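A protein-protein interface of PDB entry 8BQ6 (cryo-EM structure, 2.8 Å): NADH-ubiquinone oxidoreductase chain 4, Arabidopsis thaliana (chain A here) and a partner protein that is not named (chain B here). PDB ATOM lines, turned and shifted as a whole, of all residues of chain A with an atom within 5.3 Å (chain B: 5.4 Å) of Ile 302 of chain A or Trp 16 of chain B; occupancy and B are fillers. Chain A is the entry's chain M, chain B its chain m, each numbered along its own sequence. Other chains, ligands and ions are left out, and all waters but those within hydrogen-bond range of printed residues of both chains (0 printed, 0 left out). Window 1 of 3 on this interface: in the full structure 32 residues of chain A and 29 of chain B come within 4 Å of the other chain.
The guanidinium group (NH1) of Arg 20 of chain B is in hydrogen-bond range of the backbone carbonyl oxygen (O) of Arg 300 of chain A (3.1 Å).
O of Ile 302 of chain A lies within hydrogen-bond range of N of Val 364 of chain A, 3.0 Å away.
Ile 302 of chain A touches Trp 16 of chain B.
Ile 13 of chain B touches Leu 363 of chain A (O to CD1, 3.9 Å).
CD1 of Ile 13 of chain B touches CG of Arg 365 of chain A, at 3.96 Å.
Ile 302 of chain A touches just one residue of chain B: Trp 16 (3.7 Å).
Printed residues of chain B within 4 Å of Arg 365 of chain A: Ile 13.
Printed residues of chain A within 4 Å of Ile 13 of chain B: Leu 363 (3.9 Å) and Arg 365 (3.96 Å).
Trp 16 of chain B touches one residue of chain A.
The nearest residue of chain B that does not touch Ile 302 of chain A is Arg 20 of chain B (4.1 Å).
The nearest printed residue of chain A that does not touch Ile 13 of chain B is Ile 302 of chain A (6.3 Å).
Hydrophobic or aromatic side chains of chain A that line the printed part of chain B: Ile 302 and Leu 363.
Of the 10 printed residues of chain B, 3 touch a printed residue of chain A.
Hydrophobic or aromatic side chains of chain B within 4 Å of the printed part of chain A: Ile 13 and Trp 16.
Among the printed residues, 4 pairs touch across the chains.
Among the printed residues, no Asp or Glu carboxylate lies within 4 Å of a Lys or Arg side-chain nitrogen of the other chain.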
ATOM      1  N   ARG A 300      -1.436 -36.080 -26.041  1.00  0.00           N
ATOM      2  CA  ARG A 300      -1.899 -34.707 -25.918  1.00  0.00           C
ATOM      3  C   ARG A 300      -2.816 -34.490 -24.722  1.00  0.00           C
ATOM      4  O   ARG A 300      -3.482 -33.452 -24.647  1.00  0.00           O
ATOM      5  CB  ARG A 300      -2.605 -34.278 -27.206  1.00  0.00           C
ATOM      6  CG  ARG A 300      -1.691 -34.136 -28.414  1.00  0.00           C
ATOM      7  CD  ARG A 300      -0.471 -33.283 -28.107  1.00  0.00           C
ATOM      8  NE  ARG A 300      -0.845 -31.934 -27.700  1.00  0.00           N
ATOM      9  CZ  ARG A 300      -1.193 -30.962 -28.532  1.00  0.00           C
ATOM     10  NH1 ARG A 300      -1.152 -31.125 -29.844  1.00  0.00           N
ATOM     11  NH2 ARG A 300      -1.588 -29.793 -28.033  1.00  0.00           N
ATOM     12  N   GLN A 301      -2.861 -35.464 -23.811  1.00  0.00           N
ATOM     13  CA  GLN A 301      -3.672 -35.317 -22.574  1.00  0.00           C
ATOM     14  C   GLN A 301      -2.847 -34.589 -21.509  1.00  0.00           C
ATOM     15  O   GLN A 301      -1.620 -34.754 -21.505  1.00  0.00           O
ATOM     16  CB  GLN A 301      -4.224 -36.665 -22.101  1.00  0.00           C
ATOM     17  CG  GLN A 301      -5.140 -37.357 -23.098  1.00  0.00           C
ATOM     18  CD  GLN A 301      -6.314 -36.503 -23.507  1.00  0.00           C
ATOM     19  OE1 GLN A 301      -7.223 -36.246 -22.723  1.00  0.00           O
ATOM     20  NE2 GLN A 301      -6.304 -36.059 -24.752  1.00  0.00           N
ATOM     21  N   ILE A 302      -3.503 -33.823 -20.637  1.00  0.00           N
ATOM     22  CA  ILE A 302      -2.844 -33.000 -19.630  1.00  0.00           C
ATOM     23  C   ILE A 302      -3.219 -33.404 -18.217  1.00  0.00           C
ATOM     24  O   ILE A 302      -2.681 -32.835 -17.256  1.00  0.00           O
ATOM     25  CB  ILE A 302      -3.143 -31.509 -19.860  1.00  0.00           C
ATOM     26  CG1 ILE A 302      -4.652 -31.272 -19.819  1.00  0.00           C
ATOM     27  CG2 ILE A 302      -2.583 -31.066 -21.199  1.00  0.00           C
ATOM     28  CD1 ILE A 302      -5.054 -29.837 -19.971  1.00  0.00           C
ATOM     29  N   ASP A 303      -4.125 -34.361 -18.060  1.00  0.00           N
ATOM     30  CA  ASP A 303      -4.561 -34.875 -16.771  1.00  0.00           C
ATOM     31  C   ASP A 303      -3.845 -36.199 -16.531  1.00  0.00           C
ATOM     32  O   ASP A 303      -3.787 -37.047 -17.429  1.00  0.00           O
ATOM     33  CB  ASP A 303      -6.092 -35.037 -16.759  1.00  0.00           C
ATOM     34  CG  ASP A 303      -6.620 -35.755 -15.513  1.00  0.00           C
ATOM     35  OD1 ASP A 303      -7.821 -35.609 -15.181  1.00  0.00           O
ATOM     36  OD2 ASP A 303      -5.854 -36.465 -14.849  1.00  0.00           O
ATOM     37  N   LEU A 304      -3.310 -36.375 -15.319  1.00  0.00           N
ATOM     38  CA  LEU A 304      -2.570 -37.587 -14.978  1.00  0.00           C
ATOM     39  C   LEU A 304      -3.406 -38.838 -15.207  1.00  0.00           C
ATOM     40  O   LEU A 304      -2.950 -39.808 -15.820  1.00  0.00           O
ATOM     41  CB  LEU A 304      -2.124 -37.534 -13.518  1.00  0.00           C
ATOM     42  CG  LEU A 304      -0.848 -36.817 -13.109  1.00  0.00           C
ATOM     43  CD1 LEU A 304      -0.853 -36.676 -11.608  1.00  0.00           C
ATOM     44  CD2 LEU A 304       0.355 -37.605 -13.555  1.00  0.00           C
ATOM     45  N   ILE A 307      -4.141 -39.715 -19.020  1.00  0.00           N
ATOM     46  CA  ILE A 307      -3.020 -40.376 -19.748  1.00  0.00           C
ATOM     47  C   ILE A 307      -3.072 -41.882 -19.453  1.00  0.00           C
ATOM     48  O   ILE A 307      -3.104 -42.655 -20.416  1.00  0.00           O
ATOM     49  CB  ILE A 307      -1.675 -39.708 -19.405  1.00  0.00           C
ATOM     50  CG1 ILE A 307      -1.624 -38.275 -19.936  1.00  0.00           C
ATOM     51  CG2 ILE A 307      -0.495 -40.529 -19.903  1.00  0.00           C
ATOM     52  CD1 ILE A 307      -0.821 -37.326 -19.089  1.00  0.00           C
ATOM     53  N   ARG A 362      -4.929 -33.250 -10.542  1.00  0.00           N
ATOM     54  CA  ARG A 362      -4.519 -34.209 -11.554  1.00  0.00           C
ATOM     55  C   ARG A 362      -3.811 -33.557 -12.733  1.00  0.00           C
ATOM     56  O   ARG A 362      -3.400 -34.264 -13.657  1.00  0.00           O
ATOM     57  CB  ARG A 362      -5.732 -35.001 -12.053  1.00  0.00           C
ATOM     58  CG  ARG A 362      -6.286 -35.995 -11.049  1.00  0.00           C
ATOM     59  CD  ARG A 362      -7.195 -37.007 -11.727  1.00  0.00           C
ATOM     60  NE  ARG A 362      -8.358 -36.393 -12.355  1.00  0.00           N
ATOM     61  CZ  ARG A 362      -9.480 -36.087 -11.718  1.00  0.00           C
ATOM     62  NH1 ARG A 362      -9.629 -36.327 -10.427  1.00  0.00           N
ATOM     63  NH2 ARG A 362     -10.480 -35.530 -12.396  1.00  0.00           N
ATOM     64  N   LEU A 363      -3.649 -32.237 -12.721  1.00  0.00           N
ATOM     65  CA  LEU A 363      -3.054 -31.526 -13.846  1.00  0.00           C
ATOM     66  C   LEU A 363      -1.534 -31.645 -13.789  1.00  0.00           C
ATOM     67  O   LEU A 363      -0.917 -31.321 -12.769  1.00  0.00           O
ATOM     68  CB  LEU A 363      -3.489 -30.063 -13.829  1.00  0.00           C
ATOM     69  CG  LEU A 363      -4.938 -29.816 -14.257  1.00  0.00           C
ATOM     70  CD1 LEU A 363      -5.212 -28.340 -14.456  1.00  0.00           C
ATOM     71  CD2 LEU A 363      -5.259 -30.586 -15.521  1.00  0.00           C
ATOM     72  N   VAL A 364      -0.934 -32.096 -14.895  1.00  0.00           N
ATOM     73  CA  VAL A 364       0.507 -32.335 -14.942  1.00  0.00           C
ATOM     74  C   VAL A 364       1.291 -31.049 -14.725  1.00  0.00           C
ATOM     75  O   VAL A 364       2.401 -31.073 -14.181  1.00  0.00           O
ATOM     76  CB  VAL A 364       0.875 -33.011 -16.278  1.00  0.00           C
ATOM     77  CG1 VAL A 364       2.324 -33.409 -16.294  1.00  0.00           C
ATOM     78  CG2 VAL A 364       0.026 -34.242 -16.481  1.00  0.00           C
ATOM     79  N   ARG A 365       0.721 -29.906 -15.115  1.00  0.00           N
ATOM     80  CA  ARG A 365       1.448 -28.642 -15.055  1.00  0.00           C
ATOM     81  C   ARG A 365       1.846 -28.264 -13.633  1.00  0.00           C
ATOM     82  O   ARG A 365       2.874 -27.607 -13.433  1.00  0.00           O
ATOM     83  CB  ARG A 365       0.600 -27.532 -15.668  1.00  0.00           C
ATOM     84  CG  ARG A 365       1.377 -26.282 -15.973  1.00  0.00           C
ATOM     85  CD  ARG A 365       2.241 -26.474 -17.207  1.00  0.00           C
ATOM     86  NE  ARG A 365       3.070 -25.306 -17.484  1.00  0.00           N
ATOM     87  CZ  ARG A 365       2.602 -24.109 -17.811  1.00  0.00           C
ATOM     88  NH1 ARG A 365       1.306 -23.883 -17.947  1.00  0.00           N
ATOM     89  NH2 ARG A 365       3.459 -23.111 -18.008  1.00  0.00           N
ATOM     90  N   LYS B  11      -5.841 -19.720 -11.495  1.00  0.00           N
ATOM     91  CA  LYS B  11      -7.091 -19.545 -12.228  1.00  0.00           C
ATOM     92  C   LYS B  11      -6.897 -19.772 -13.722  1.00  0.00           C
ATOM     93  O   LYS B  11      -7.773 -20.331 -14.393  1.00  0.00           O
ATOM     94  CB  LYS B  11      -7.664 -18.153 -11.957  1.00  0.00           C
ATOM     95  CG  LYS B  11      -8.450 -17.552 -13.114  1.00  0.00           C
ATOM     96  CD  LYS B  11      -8.773 -16.085 -12.872  1.00  0.00           C
ATOM     97  CE  LYS B  11      -7.703 -15.177 -13.437  1.00  0.00           C
ATOM     98  NZ  LYS B  11      -7.938 -14.960 -14.887  1.00  0.00           N
ATOM     99  N   PHE B  12      -5.744 -19.356 -14.252  1.00  0.00           N
ATOM    100  CA  PHE B  12      -5.466 -19.497 -15.707  1.00  0.00           C
ATOM    101  C   PHE B  12      -5.205 -20.969 -16.046  1.00  0.00           C
ATOM    102  O   PHE B  12      -5.669 -21.420 -17.109  1.00  0.00           O
ATOM    103  CB  PHE B  12      -4.282 -18.620 -16.126  1.00  0.00           C
ATOM    104  CG  PHE B  12      -4.330 -17.210 -15.598  1.00  0.00           C
ATOM    105  CD1 PHE B  12      -4.910 -16.199 -16.342  1.00  0.00           C
ATOM    106  CD2 PHE B  12      -3.808 -16.894 -14.353  1.00  0.00           C
ATOM    107  CE1 PHE B  12      -4.955 -14.902 -15.859  1.00  0.00           C
ATOM    108  CE2 PHE B  12      -3.866 -15.599 -13.864  1.00  0.00           C
ATOM    109  CZ  PHE B  12      -4.438 -14.604 -14.619  1.00  0.00           C
ATOM    110  N   ILE B  13      -4.480 -21.686 -15.178  1.00  0.00           N
ATOM    111  CA  ILE B  13      -4.170 -23.085 -15.462  1.00  0.00           C
ATOM    112  C   ILE B  13      -5.425 -23.941 -15.337  1.00  0.00           C
ATOM    113  O   ILE B  13      -5.648 -24.865 -16.130  1.00  0.00           O
ATOM    114  CB  ILE B  13      -3.035 -23.582 -14.548  1.00  0.00           C
ATOM    115  CG1 ILE B  13      -1.697 -23.004 -15.012  1.00  0.00           C
ATOM    116  CG2 ILE B  13      -2.951 -25.090 -14.564  1.00  0.00           C
ATOM    117  CD1 ILE B  13      -0.538 -23.354 -14.114  1.00  0.00           C
ATOM    118  N   GLU B  14      -6.272 -23.639 -14.351  1.00  0.00           N
ATOM    119  CA  GLU B  14      -7.524 -24.374 -14.196  1.00  0.00           C
ATOM    120  C   GLU B  14      -8.488 -24.098 -15.343  1.00  0.00           C
ATOM    121  O   GLU B  14      -9.195 -25.006 -15.797  1.00  0.00           O
ATOM    122  CB  GLU B  14      -8.163 -24.032 -12.854  1.00  0.00           C
ATOM    123  CG  GLU B  14      -9.170 -25.061 -12.374  1.00  0.00           C
ATOM    124  CD  GLU B  14      -8.554 -26.068 -11.431  1.00  0.00           C
ATOM    125  OE1 GLU B  14      -8.942 -27.253 -11.475  1.00  0.00           O
ATOM    126  OE2 GLU B  14      -7.646 -25.678 -10.677  1.00  0.00           O
ATOM    127  N   ASP B  15      -8.549 -22.849 -15.813  1.00  0.00           N
ATOM    128  CA  ASP B  15      -9.376 -22.528 -16.974  1.00  0.00           C
ATOM    129  C   ASP B  15      -8.932 -23.314 -18.194  1.00  0.00           C
ATOM    130  O   ASP B  15      -9.760 -23.832 -18.954  1.00  0.00           O
ATOM    131  CB  ASP B  15      -9.302 -21.034 -17.267  1.00  0.00           C
ATOM    132  CG  ASP B  15     -10.316 -20.245 -16.491  1.00  0.00           C
ATOM    133  OD1 ASP B  15     -10.840 -20.781 -15.495  1.00  0.00           O
ATOM    134  OD2 ASP B  15     -10.585 -19.087 -16.870  1.00  0.00           O
ATOM    135  N   TRP B  16      -7.612 -23.424 -18.380  1.00  0.00           N
ATOM    136  CA  TRP B  16      -7.076 -24.265 -19.480  1.00  0.00           C
ATOM    137  C   TRP B  16      -7.540 -25.708 -19.255  1.00  0.00           C
ATOM    138  O   TRP B  16      -7.908 -26.363 -20.242  1.00  0.00           O
ATOM    139  CB  TRP B  16      -5.548 -24.155 -19.522  1.00  0.00           C
ATOM    140  CG  TRP B  16      -4.863 -24.883 -20.633  1.00  0.00           C
ATOM    141  CD1 TRP B  16      -5.139 -24.821 -21.968  1.00  0.00           C
ATOM    142  CD2 TRP B  16      -3.739 -25.767 -20.497  1.00  0.00           C
ATOM    143  NE1 TRP B  16      -4.276 -25.619 -22.669  1.00  0.00           N
ATOM    144  CE2 TRP B  16      -3.404 -26.209 -21.794  1.00  0.00           C
ATOM    145  CE3 TRP B  16      -2.994 -26.231 -19.408  1.00  0.00           C
ATOM    146  CZ2 TRP B  16      -2.355 -27.095 -22.024  1.00  0.00           C
ATOM    147  CZ3 TRP B  16      -1.956 -27.104 -19.638  1.00  0.00           C
ATOM    148  CH2 TRP B  16      -1.642 -27.526 -20.930  1.00  0.00           C
ATOM    149  N   GLY B  17      -7.551 -26.163 -17.993  1.00  0.00           N
ATOM    150  CA  GLY B  17      -7.966 -27.531 -17.727  1.00  0.00           C
ATOM    151  C   GLY B  17      -9.432 -27.777 -18.034  1.00  0.00           C
ATOM    152  O   GLY B  17      -9.794 -28.803 -18.613  1.00  0.00           O
ATOM    153  N   SER B  18     -10.298 -26.838 -17.645  1.00  0.00           N
ATOM    154  CA  SER B  18     -11.727 -27.027 -17.874  1.00  0.00           C
ATOM    155  C   SER B  18     -12.094 -26.882 -19.345  1.00  0.00           C
ATOM    156  O   SER B  18     -13.023 -27.548 -19.817  1.00  0.00           O
ATOM    157  CB  SER B  18     -12.536 -26.039 -17.035  1.00  0.00           C
ATOM    158  OG  SER B  18     -11.998 -24.735 -17.131  1.00  0.00           O
ATOM    159  N   ALA B  19     -11.400 -26.012 -20.079  1.00  0.00           N
ATOM    160  CA  ALA B  19     -11.701 -25.855 -21.497  1.00  0.00           C
ATOM    161  C   ALA B  19     -11.337 -27.113 -22.275  1.00  0.00           C
ATOM    162  O   ALA B  19     -11.934 -27.402 -23.319  1.00  0.00           O
ATOM    163  CB  ALA B  19     -10.969 -24.638 -22.061  1.00  0.00           C
ATOM    164  N   ARG B  20     -10.350 -27.868 -21.789  1.00  0.00           N
ATOM    165  CA  ARG B  20     -10.013 -29.138 -22.420  1.00  0.00           C
ATOM    166  C   ARG B  20     -11.103 -30.178 -22.213  1.00  0.00           C
ATOM    167  O   ARG B  20     -11.464 -30.906 -23.145  1.00  0.00           O
ATOM    168  CB  ARG B  20      -8.693 -29.664 -21.874  1.00  0.00           C
ATOM    169  CG  ARG B  20      -8.283 -30.942 -22.527  1.00  0.00           C
ATOM    170  CD  ARG B  20      -8.190 -30.748 -24.011  1.00  0.00           C
ATOM    171  NE  ARG B  20      -7.262 -29.676 -24.327  1.00  0.00           N
ATOM    172  CZ  ARG B  20      -5.952 -29.832 -24.439  1.00  0.00           C
ATOM    173  NH1 ARG B  20      -5.382 -31.013 -24.281  1.00  0.00           N
ATOM    174  NH2 ARG B  20      -5.200 -28.776 -24.722  1.00  0.00           N
